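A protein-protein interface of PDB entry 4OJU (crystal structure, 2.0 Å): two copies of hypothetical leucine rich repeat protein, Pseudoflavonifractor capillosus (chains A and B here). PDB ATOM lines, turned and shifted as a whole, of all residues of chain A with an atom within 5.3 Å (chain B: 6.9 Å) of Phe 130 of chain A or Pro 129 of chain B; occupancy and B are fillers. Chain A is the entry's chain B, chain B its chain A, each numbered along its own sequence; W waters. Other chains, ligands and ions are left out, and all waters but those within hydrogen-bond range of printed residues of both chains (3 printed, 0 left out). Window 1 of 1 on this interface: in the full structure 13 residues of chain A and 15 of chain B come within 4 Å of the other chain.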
ATOM      1  N   ASN A 128      -0.623  -3.576  10.406  1.00  0.00           N
ATOM      2  CA  ASN A 128       0.239  -3.145   9.289  1.00  0.00           C
ATOM      3  C   ASN A 128       1.004  -1.884   9.751  1.00  0.00           C
ATOM      4  O   ASN A 128       0.375  -0.863   9.985  1.00  0.00           O
ATOM      5  CB  ASN A 128      -0.615  -2.876   8.032  1.00  0.00           C
ATOM      6  CG  ASN A 128       0.144  -2.262   6.884  1.00  0.00           C
ATOM      7  OD1 ASN A 128       1.354  -2.058   6.941  1.00  0.00           O
ATOM      8  ND2 ASN A 128      -0.565  -1.878   5.855  1.00  0.00           N
ATOM      9  N   PRO A 129       2.338  -1.961   9.949  1.00  0.00           N
ATOM     10  CA  PRO A 129       3.062  -0.815  10.513  1.00  0.00           C
ATOM     11  C   PRO A 129       3.114   0.411   9.612  1.00  0.00           C
ATOM     12  O   PRO A 129       3.323   1.511  10.116  1.00  0.00           O
ATOM     13  CB  PRO A 129       4.467  -1.372  10.778  1.00  0.00           C
ATOM     14  CG  PRO A 129       4.605  -2.515   9.849  1.00  0.00           C
ATOM     15  CD  PRO A 129       3.235  -3.112   9.729  1.00  0.00           C
ATOM     16  N   PHE A 130       2.901   0.242   8.298  1.00  0.00           N
ATOM     17  CA  PHE A 130       2.931   1.379   7.389  1.00  0.00           C
ATOM     18  C   PHE A 130       1.694   2.277   7.567  1.00  0.00           C
ATOM     19  O   PHE A 130       1.693   3.392   7.067  1.00  0.00           O
ATOM     20  CB  PHE A 130       3.079   0.896   5.930  1.00  0.00           C
ATOM     21  CG  PHE A 130       4.386   0.156   5.740  1.00  0.00           C
ATOM     22  CD1 PHE A 130       5.584   0.852   5.592  1.00  0.00           C
ATOM     23  CD2 PHE A 130       4.424  -1.236   5.751  1.00  0.00           C
ATOM     24  CE1 PHE A 130       6.798   0.166   5.412  1.00  0.00           C
ATOM     25  CE2 PHE A 130       5.648  -1.923   5.631  1.00  0.00           C
ATOM     26  CZ  PHE A 130       6.817  -1.219   5.438  1.00  0.00           C
ATOM     27  N   ARG A 131       0.668   1.818   8.322  1.00  0.00           N
ATOM     28  CA  ARG A 131      -0.516   2.657   8.627  1.00  0.00           C
ATOM     29  C   ARG A 131      -0.177   3.706   9.681  1.00  0.00           C
ATOM     30  O   ARG A 131      -0.915   4.679   9.839  1.00  0.00           O
ATOM     31  CB  ARG A 131      -1.662   1.776   9.220  1.00  0.00           C
ATOM     32  CG  ARG A 131      -2.249   0.689   8.324  1.00  0.00           C
ATOM     33  CD  ARG A 131      -3.241  -0.113   9.178  1.00  0.00           C
ATOM     34  NE  ARG A 131      -4.569   0.493   9.148  1.00  0.00           N
ATOM     35  CZ  ARG A 131      -5.540   0.275  10.032  1.00  0.00           C
ATOM     36  NH1 ARG A 131      -5.324  -0.500  11.091  1.00  0.00           N
ATOM     37  NH2 ARG A 131      -6.725   0.839   9.873  1.00  0.00           N
ATOM     38  N   TRP A 132       0.888   3.469  10.457  1.00  0.00           N
ATOM     39  CA  TRP A 132       1.264   4.313  11.600  1.00  0.00           C
ATOM     40  C   TRP A 132       1.832   5.670  11.238  1.00  0.00           C
ATOM     41  O   TRP A 132       1.419   6.668  11.814  1.00  0.00           O
ATOM     42  CB  TRP A 132       2.272   3.596  12.511  1.00  0.00           C
ATOM     43  CG  TRP A 132       1.799   2.253  13.004  1.00  0.00           C
ATOM     44  CD1 TRP A 132       0.508   1.821  13.123  1.00  0.00           C
ATOM     45  CD2 TRP A 132       2.624   1.200  13.499  1.00  0.00           C
ATOM     46  NE1 TRP A 132       0.481   0.549  13.649  1.00  0.00           N
ATOM     47  CE2 TRP A 132       1.770   0.139  13.882  1.00  0.00           C
ATOM     48  CE3 TRP A 132       4.019   1.026  13.611  1.00  0.00           C
ATOM     49  CZ2 TRP A 132       2.262  -1.089  14.333  1.00  0.00           C
ATOM     50  CZ3 TRP A 132       4.503  -0.180  14.094  1.00  0.00           C
ATOM     51  CH2 TRP A 132       3.633  -1.210  14.467  1.00  0.00           C
ATOM     52  N   SER A 133       2.767   5.712  10.294  1.00  0.00           N
ATOM     53  CA  SER A 133       3.472   6.945   9.993  1.00  0.00           C
ATOM     54  C   SER A 133       3.591   7.172   8.518  1.00  0.00           C
ATOM     55  O   SER A 133       3.967   6.265   7.771  1.00  0.00           O
ATOM     56  CB  SER A 133       4.867   6.902  10.617  1.00  0.00           C
ATOM     57  OG  SER A 133       5.712   7.889  10.054  1.00  0.00           O
ATOM     58  N   LEU A 136       7.227   6.675   7.378  1.00  0.00           N
ATOM     59  CA  LEU A 136       7.811   5.339   7.530  1.00  0.00           C
ATOM     60  C   LEU A 136       7.864   4.627   6.180  1.00  0.00           C
ATOM     61  O   LEU A 136       6.906   3.971   5.774  1.00  0.00           O
ATOM     62  CB  LEU A 136       6.986   4.529   8.553  1.00  0.00           C
ATOM     63  CG  LEU A 136       7.525   3.149   8.975  1.00  0.00           C
ATOM     64  CD1 LEU A 136       8.842   3.263   9.683  1.00  0.00           C
ATOM     65  CD2 LEU A 136       6.543   2.447   9.910  1.00  0.00           C
ATOM     66  N   ASP A 137       8.958   4.778   5.475  1.00  0.00           N
ATOM     67  CA  ASP A 137       9.112   4.172   4.150  1.00  0.00           C
ATOM     68  C   ASP A 137       9.469   2.691   4.196  1.00  0.00           C
ATOM     69  O   ASP A 137       9.066   1.942   3.297  1.00  0.00           O
ATOM     70  CB  ASP A 137      10.219   4.890   3.376  1.00  0.00           C
ATOM     71  CG  ASP A 137       9.882   6.325   2.980  1.00  0.00           C
ATOM     72  OD1 ASP A 137       8.690   6.702   3.062  1.00  0.00           O
ATOM     73  OD2 ASP A 137      10.799   7.047   2.542  1.00  0.00           O
ATOM     74  N   THR A 138      10.265   2.297   5.198  1.00  0.00           N
ATOM     75  CA  THR A 138      10.783   0.937   5.338  1.00  0.00           C
ATOM     76  C   THR A 138      10.680   0.436   6.782  1.00  0.00           C
ATOM     77  O   THR A 138      10.921   1.192   7.730  1.00  0.00           O
ATOM     78  CB  THR A 138      12.250   0.937   4.842  1.00  0.00           C
ATOM     79  OG1 THR A 138      12.267   1.366   3.487  1.00  0.00           O
ATOM     80  CG2 THR A 138      12.935  -0.413   4.955  1.00  0.00           C
ATOM     81  N   VAL A 139      10.367  -0.865   6.934  1.00  0.00           N
ATOM     82  CA  VAL A 139      10.292  -1.547   8.209  1.00  0.00           C
ATOM     83  C   VAL A 139      11.366  -2.642   8.167  1.00  0.00           C
ATOM     84  O   VAL A 139      11.449  -3.372   7.172  1.00  0.00           O
ATOM     85  CB  VAL A 139       8.873  -2.104   8.503  1.00  0.00           C
ATOM     86  CG1 VAL A 139       8.870  -3.001   9.741  1.00  0.00           C
ATOM     87  CG2 VAL A 139       7.878  -0.962   8.678  1.00  0.00           C
ATOM     88  N   ILE B 103      11.024  -7.380   0.358  1.00  0.00           N
ATOM     89  CA  ILE B 103       9.735  -7.100  -0.263  1.00  0.00           C
ATOM     90  C   ILE B 103       9.816  -5.645  -0.667  1.00  0.00           C
ATOM     91  O   ILE B 103       9.869  -4.765   0.207  1.00  0.00           O
ATOM     92  CB  ILE B 103       8.495  -7.435   0.594  1.00  0.00           C
ATOM     93  CG1 ILE B 103       8.584  -8.894   1.147  1.00  0.00           C
ATOM     94  CG2 ILE B 103       7.223  -7.229  -0.286  1.00  0.00           C
ATOM     95  CD1 ILE B 103       7.387  -9.347   2.105  1.00  0.00           C
ATOM     96  N   ASN B 104       9.933  -5.397  -1.980  1.00  0.00           N
ATOM     97  CA  ASN B 104      10.125  -4.048  -2.505  1.00  0.00           C
ATOM     98  C   ASN B 104       8.866  -3.242  -2.483  1.00  0.00           C
ATOM     99  O   ASN B 104       7.777  -3.750  -2.239  1.00  0.00           O
ATOM    100  CB  ASN B 104      10.717  -4.066  -3.907  1.00  0.00           C
ATOM    101  CG  ASN B 104      12.199  -4.303  -3.861  1.00  0.00           C
ATOM    102  OD1 ASN B 104      12.988  -3.387  -3.681  1.00  0.00           O
ATOM    103  ND2 ASN B 104      12.601  -5.537  -3.909  1.00  0.00           N
ATOM    104  N   GLU B 105       9.028  -1.951  -2.741  1.00  0.00           N
ATOM    105  CA  GLU B 105       7.973  -0.974  -2.637  1.00  0.00           C
ATOM    106  C   GLU B 105       6.713  -1.380  -3.410  1.00  0.00           C
ATOM    107  O   GLU B 105       6.775  -1.805  -4.570  1.00  0.00           O
ATOM    108  CB  GLU B 105       8.499   0.404  -3.059  1.00  0.00           C
ATOM    109  CG  GLU B 105       7.952   1.021  -4.330  1.00  0.00           C
ATOM    110  CD  GLU B 105       8.582   2.351  -4.704  1.00  0.00           C
ATOM    111  OE1 GLU B 105       9.184   3.010  -3.826  1.00  0.00           O
ATOM    112  OE2 GLU B 105       8.480   2.730  -5.888  1.00  0.00           O
ATOM    113  N   LEU B 106       5.565  -1.264  -2.734  1.00  0.00           N
ATOM    114  CA  LEU B 106       4.250  -1.458  -3.316  1.00  0.00           C
ATOM    115  C   LEU B 106       4.055  -2.849  -3.964  1.00  0.00           C
ATOM    116  O   LEU B 106       3.196  -2.997  -4.841  1.00  0.00           O
ATOM    117  CB  LEU B 106       4.011  -0.344  -4.360  1.00  0.00           C
ATOM    118  CG  LEU B 106       4.152   1.105  -3.894  1.00  0.00           C
ATOM    119  CD1 LEU B 106       4.113   2.066  -5.094  1.00  0.00           C
ATOM    120  CD2 LEU B 106       3.052   1.439  -2.936  1.00  0.00           C
ATOM    121  N   ALA B 107       4.811  -3.862  -3.537  1.00  0.00           N
ATOM    122  CA  ALA B 107       4.744  -5.220  -4.118  1.00  0.00           C
ATOM    123  C   ALA B 107       3.331  -5.823  -4.022  1.00  0.00           C
ATOM    124  O   ALA B 107       2.922  -6.549  -4.918  1.00  0.00           O
ATOM    125  CB  ALA B 107       5.748  -6.135  -3.430  1.00  0.00           C
ATOM    126  N   PHE B 108       2.569  -5.482  -2.966  1.00  0.00           N
ATOM    127  CA  PHE B 108       1.193  -5.976  -2.820  1.00  0.00           C
ATOM    128  C   PHE B 108       0.262  -4.774  -2.692  1.00  0.00           C
ATOM    129  O   PHE B 108      -0.669  -4.777  -1.882  1.00  0.00           O
ATOM    130  CB  PHE B 108       1.078  -6.925  -1.593  1.00  0.00           C
ATOM    131  CG  PHE B 108       1.873  -8.195  -1.768  1.00  0.00           C
ATOM    132  CD1 PHE B 108       1.348  -9.269  -2.478  1.00  0.00           C
ATOM    133  CD2 PHE B 108       3.167  -8.299  -1.266  1.00  0.00           C
ATOM    134  CE1 PHE B 108       2.093 -10.438  -2.656  1.00  0.00           C
ATOM    135  CE2 PHE B 108       3.919  -9.465  -1.461  1.00  0.00           C
ATOM    136  CZ  PHE B 108       3.385 -10.513  -2.178  1.00  0.00           C
ATOM    137  N   ALA B 109       0.525  -3.728  -3.477  1.00  0.00           N
ATOM    138  CA  ALA B 109      -0.248  -2.490  -3.398  1.00  0.00           C
ATOM    139  C   ALA B 109      -1.606  -2.583  -4.071  1.00  0.00           C
ATOM    140  O   ALA B 109      -1.751  -3.242  -5.102  1.00  0.00           O
ATOM    141  CB  ALA B 109       0.535  -1.338  -4.011  1.00  0.00           C
ATOM    142  N   SER B 110      -2.603  -1.890  -3.496  1.00  0.00           N
ATOM    143  CA  SER B 110      -3.973  -1.827  -4.031  1.00  0.00           C
ATOM    144  C   SER B 110      -4.545  -3.232  -4.411  1.00  0.00           C
ATOM    145  O   SER B 110      -5.082  -3.420  -5.513  1.00  0.00           O
ATOM    146  CB  SER B 110      -4.000  -0.885  -5.240  1.00  0.00           C
ATOM    147  OG  SER B 110      -5.298  -0.662  -5.764  1.00  0.00           O
ATOM    148  N   CYS B 111      -4.377  -4.213  -3.502  1.00  0.00           N
ATOM    149  CA  CYS B 111      -4.903  -5.586  -3.592  1.00  0.00           C
ATOM    150  C   CYS B 111      -6.038  -5.623  -2.598  1.00  0.00           C
ATOM    151  O   CYS B 111      -5.842  -5.976  -1.435  1.00  0.00           O
ATOM    152  CB  CYS B 111      -3.817  -6.614  -3.255  1.00  0.00           C
ATOM    153  SG  CYS B 111      -2.540  -6.773  -4.518  1.00  0.00           S
ATOM    154  N   ILE B 119       4.488 -13.136   7.059  1.00  0.00           N
ATOM    155  CA  ILE B 119       5.849 -12.786   6.679  1.00  0.00           C
ATOM    156  C   ILE B 119       6.807 -13.838   7.211  1.00  0.00           C
ATOM    157  O   ILE B 119       6.874 -14.062   8.419  1.00  0.00           O
ATOM    158  CB  ILE B 119       6.203 -11.359   7.202  1.00  0.00           C
ATOM    159  CG1 ILE B 119       5.206 -10.276   6.739  1.00  0.00           C
ATOM    160  CG2 ILE B 119       7.639 -10.954   6.886  1.00  0.00           C
ATOM    161  CD1 ILE B 119       4.997 -10.059   5.199  1.00  0.00           C
ATOM    162  N   LYS B 125      13.701  -6.792   5.376  1.00  0.00           N
ATOM    163  CA  LYS B 125      13.303  -5.441   5.021  1.00  0.00           C
ATOM    164  C   LYS B 125      12.084  -5.440   4.108  1.00  0.00           C
ATOM    165  O   LYS B 125      12.018  -6.193   3.134  1.00  0.00           O
ATOM    166  CB  LYS B 125      14.511  -4.791   4.285  1.00  0.00           C
ATOM    167  CG  LYS B 125      14.410  -3.329   3.926  1.00  0.00           C
ATOM    168  CD  LYS B 125      15.682  -2.902   3.181  1.00  0.00           C
ATOM    169  CE  LYS B 125      15.515  -1.616   2.416  1.00  0.00           C
ATOM    170  NZ  LYS B 125      16.670  -1.368   1.514  1.00  0.00           N
ATOM    171  N   MET B 126      11.169  -4.503   4.394  1.00  0.00           N
ATOM    172  CA  MET B 126       9.955  -4.251   3.610  1.00  0.00           C
ATOM    173  C   MET B 126       9.816  -2.769   3.330  1.00  0.00           C
ATOM    174  O   MET B 126       9.818  -1.996   4.286  1.00  0.00           O
ATOM    175  CB  MET B 126       8.693  -4.732   4.360  1.00  0.00           C
ATOM    176  CG  MET B 126       8.670  -6.235   4.620  1.00  0.00           C
ATOM    177  SD  MET B 126       6.941  -6.731   5.385  1.00  0.00           S
ATOM    178  CE  MET B 126       6.750  -5.481   6.870  1.00  0.00           C
ATOM    179  N   ASP B 127       9.723  -2.372   2.037  1.00  0.00           N
ATOM    180  CA  ASP B 127       9.455  -0.979   1.596  1.00  0.00           C
ATOM    181  C   ASP B 127       7.953  -0.902   1.300  1.00  0.00           C
ATOM    182  O   ASP B 127       7.535  -1.576   0.370  1.00  0.00           O
ATOM    183  CB  ASP B 127      10.300  -0.647   0.345  1.00  0.00           C
ATOM    184  CG  ASP B 127      11.793  -0.880   0.493  1.00  0.00           C
ATOM    185  OD1 ASP B 127      12.246  -1.103   1.616  1.00  0.00           O
ATOM    186  OD2 ASP B 127      12.499  -0.861  -0.528  1.00  0.00           O
ATOM    187  N   ASN B 128       7.121  -0.198   2.140  1.00  0.00           N
ATOM    188  CA  ASN B 128       5.624  -0.153   2.115  1.00  0.00           C
ATOM    189  C   ASN B 128       4.995  -0.976   0.961  1.00  0.00           C
ATOM    190  O   ASN B 128       4.614  -0.444  -0.084  1.00  0.00           O
ATOM    191  CB  ASN B 128       5.038   1.256   2.142  1.00  0.00           C
ATOM    192  CG  ASN B 128       3.549   1.262   2.462  1.00  0.00           C
ATOM    193  OD1 ASN B 128       2.891   0.217   2.641  1.00  0.00           O
ATOM    194  ND2 ASN B 128       2.985   2.430   2.579  1.00  0.00           N
ATOM    195  N   PRO B 129       4.901  -2.306   1.147  1.00  0.00           N
ATOM    196  CA  PRO B 129       4.369  -3.154   0.070  1.00  0.00           C
ATOM    197  C   PRO B 129       2.847  -3.175   0.012  1.00  0.00           C
ATOM    198  O   PRO B 129       2.310  -3.685  -0.949  1.00  0.00           O
ATOM    199  CB  PRO B 129       4.883  -4.561   0.451  1.00  0.00           C
ATOM    200  CG  PRO B 129       5.932  -4.319   1.576  1.00  0.00           C
ATOM    201  CD  PRO B 129       5.378  -3.131   2.278  1.00  0.00           C
ATOM    202  N   PHE B 130       2.154  -2.703   1.048  1.00  0.00           N
ATOM    203  CA  PHE B 130       0.703  -2.867   1.159  1.00  0.00           C
ATOM    204  C   PHE B 130      -0.105  -1.580   0.999  1.00  0.00           C
ATOM    205  O   PHE B 130      -1.319  -1.591   1.241  1.00  0.00           O
ATOM    206  CB  PHE B 130       0.413  -3.506   2.521  1.00  0.00           C
ATOM    207  CG  PHE B 130       1.369  -4.655   2.823  1.00  0.00           C
ATOM    208  CD1 PHE B 130       1.345  -5.820   2.063  1.00  0.00           C
ATOM    209  CD2 PHE B 130       2.249  -4.587   3.899  1.00  0.00           C
ATOM    210  CE1 PHE B 130       2.224  -6.873   2.337  1.00  0.00           C
ATOM    211  CE2 PHE B 130       3.123  -5.639   4.172  1.00  0.00           C
ATOM    212  CZ  PHE B 130       3.108  -6.770   3.383  1.00  0.00           C
ATOM    213  N   ARG B 131       0.535  -0.496   0.525  1.00  0.00           N
ATOM    214  CA  ARG B 131      -0.150   0.787   0.329  1.00  0.00           C
ATOM    215  C   ARG B 131      -1.401   0.609  -0.528  1.00  0.00           C
ATOM    216  O   ARG B 131      -1.352  -0.125  -1.521  1.00  0.00           O
ATOM    217  CB  ARG B 131       0.784   1.817  -0.321  1.00  0.00           C
ATOM    218  CG  ARG B 131       0.289   3.265  -0.166  1.00  0.00           C
ATOM    219  CD  ARG B 131       1.394   4.218  -0.557  1.00  0.00           C
ATOM    220  NE  ARG B 131       0.958   5.612  -0.536  1.00  0.00           N
ATOM    221  CZ  ARG B 131       1.725   6.641  -0.893  1.00  0.00           C
ATOM    222  NH1 ARG B 131       2.982   6.443  -1.259  1.00  0.00           N
ATOM    223  NH2 ARG B 131       1.244   7.875  -0.865  1.00  0.00           N
ATOM    224  N   SER B 133      -3.933  -1.148  -0.136  1.00  0.00           N
ATOM    225  CA  SER B 133      -4.628  -2.424  -0.003  1.00  0.00           C
ATOM    226  C   SER B 133      -5.527  -2.301   1.233  1.00  0.00           C
ATOM    227  O   SER B 133      -5.077  -2.518   2.365  1.00  0.00           O
ATOM    228  CB  SER B 133      -3.650  -3.585   0.101  1.00  0.00           C
ATOM    229  OG  SER B 133      -2.949  -3.708  -1.122  1.00  0.00           O
ATOM    230  N   LEU B 136      -5.989  -5.030   4.146  1.00  0.00           N
ATOM    231  CA  LEU B 136      -4.767  -5.585   4.708  1.00  0.00           C
ATOM    232  C   LEU B 136      -4.429  -4.919   6.036  1.00  0.00           C
ATOM    233  O   LEU B 136      -3.564  -4.043   6.121  1.00  0.00           O
ATOM    234  CB  LEU B 136      -3.608  -5.485   3.715  1.00  0.00           C
ATOM    235  CG  LEU B 136      -2.380  -6.355   3.975  1.00  0.00           C
ATOM    236  CD1 LEU B 136      -2.700  -7.643   4.741  1.00  0.00           C
ATOM    237  CD2 LEU B 136      -1.761  -6.691   2.697  1.00  0.00           C
HETATM  238  O   HOH W   1       0.435  -0.081   3.710  1.00  0.00           O
HETATM  239  O   HOH W   2       5.176   4.938   3.332  1.00  0.00           O
HETATM  240  O   HOH W   3       8.366   2.705   0.669  1.00  0.00           O
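N of Asn 128 of chain B lies within hydrogen-bond range of O of Asp 137 of chain A. The side-chain hydroxyl of Thr 138 of chain A is in hydrogen-bond range of the side-chain carboxylate of Asp 127 of chain B. O of Met 126 of chain B sits at hydrogen-bond distance from N of Val 139 of chain A (2.9 Å).
Printed residues of chain B within 4 Å of Asn 128 of chain A: Phe 130 (3.8 Å) and Leu 136 (3.7 Å). Phe 130 of chain A touches just these residues of chain B: Met 126, Asn 128 and Pro 129. Of the printed residues of chain B, Thr 138 of chain A touches Lys 125, Met 126 and Asp 127. Glu 105 of chain B touches none of the printed residues of chain A. Ala 107 of chain B touches none of the printed residues of chain A. Of the printed residues of chain A, Met 126 of chain B touches Phe 130 (3.3 Å), Thr 138 (3.3 Å) and Val 139 (2.9 Å). Of the printed residues of chain A, Asn 128 of chain B touches Phe 130 and Asp 137. Of chain A, only Phe 130 (3.6 Å) comes within 4 Å of Pro 129 of chain B. Of the printed residues of chain A, Leu 136 of chain B touches Asn 128. The nearest printed residue of chain A that does not touch Pro 129 of chain B is Asn 128 of chain A (6.3 Å). The nearest printed residue of chain B that does not touch Thr 138 of chain A is Asn 128 of chain B (5.0 Å).
Asn 128 of chain A touches Phe 130 of chain B, and with the chains exchanged Phe 130 of chain A touches Asn 128 of chain B. Asn 128 of chain A touches Leu 136 of chain B, but with the chains exchanged Leu 136 of chain A does not touch Asn 128 of chain B (4.9 Å). Phe 130 of chain A touches Pro 129 of chain B, but with the chains exchanged Pro 129 of chain A does not touch Phe 130 of chain B (6.1 Å). 6 positions are printed for both chains. Of the 12 pairs that touch across the chains among the printed residues, 2 have their exchanged pair printed and touching as well.
The backbone NH (N) of Asp 127 of chain B sits at hydrogen-bond distance from the backbone carbonyl oxygen (O) of Ile 103 of chain B, at 3.0 Å. The backbone carbonyl oxygen of Pro 129 of chain B is in hydrogen-bond range of the backbone NH of Ala 109 of chain B, 3.1 Å away. The backbone NH of Phe 108 of chain B is in hydrogen-bond range of the backbone carbonyl oxygen of Pro 129 of chain B, at 2.7 Å. N of Leu 106 of chain B is in hydrogen-bond range of O of Asn 128 of chain B (2.9 Å). The side-chain amide oxygen (OD1) of Asn 128 of chain B is in hydrogen-bond range of the backbone NH (N) of Arg 131 of chain B (3.2 Å). OD1 of Asn 128 of chain A lies within hydrogen-bond range of N of Phe 130 of chain A, at 3.1 Å.
Of the 10 printed residues of chain A, 5 touch a printed residue of chain B. Printed residues of chain B that touch a printed residue of chain A: Lys 125, Met 126, Asp 127, Asn 128, Pro 129, Phe 130 and Leu 136. Hydrophobic or aromatic side chains of chain B that line the printed part of chain A: Met 126, Pro 129 and Phe 130.
Water W1 lies within hydrogen-bond range of the side-chain amide oxygen of Asn 128 of chain B (2.7 Å), the side-chain amide nitrogen of Asn 128 of chain A (3.0 Å), the backbone NH of Arg 131 of chain B (3.2 Å) and the backbone carbonyl oxygen of Phe 130 of chain B (3.4 Å). Water W3 lies within hydrogen-bond range of O of Asp 137 of chain A (2.8 Å) and N of Asn 128 of chain B (3.5 Å). Water W2 lies within hydrogen-bond range of O of Leu 136 of chain A (3.1 Å) and ND2 of Asn 128 of chain B (3.4 Å).
Among the printed residues, merely in contact across the chains: Thr 138 of chain A with Met 126 of chain B (3.3 Å), Phe 130 of chain A with Met 126 of chain B (3.3 Å), Phe 130 of chain A with Asn 128 of chain B (3.3 Å), Asp 137 of chain A with Asp 127 of chain B (3.4 Å), Thr 138 of chain A with Lys 125 of chain B (3.4 Å), Val 139 of chain A with Lys 125 of chain B (3.5 Å), Phe 130 of chain A with Pro 129 of chain B (3.6 Å), Asn 128 of chain A with Leu 136 of chain B (3.7 Å) and Asn 128 of chain A with Phe 130 of chain B (3.8 Å).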
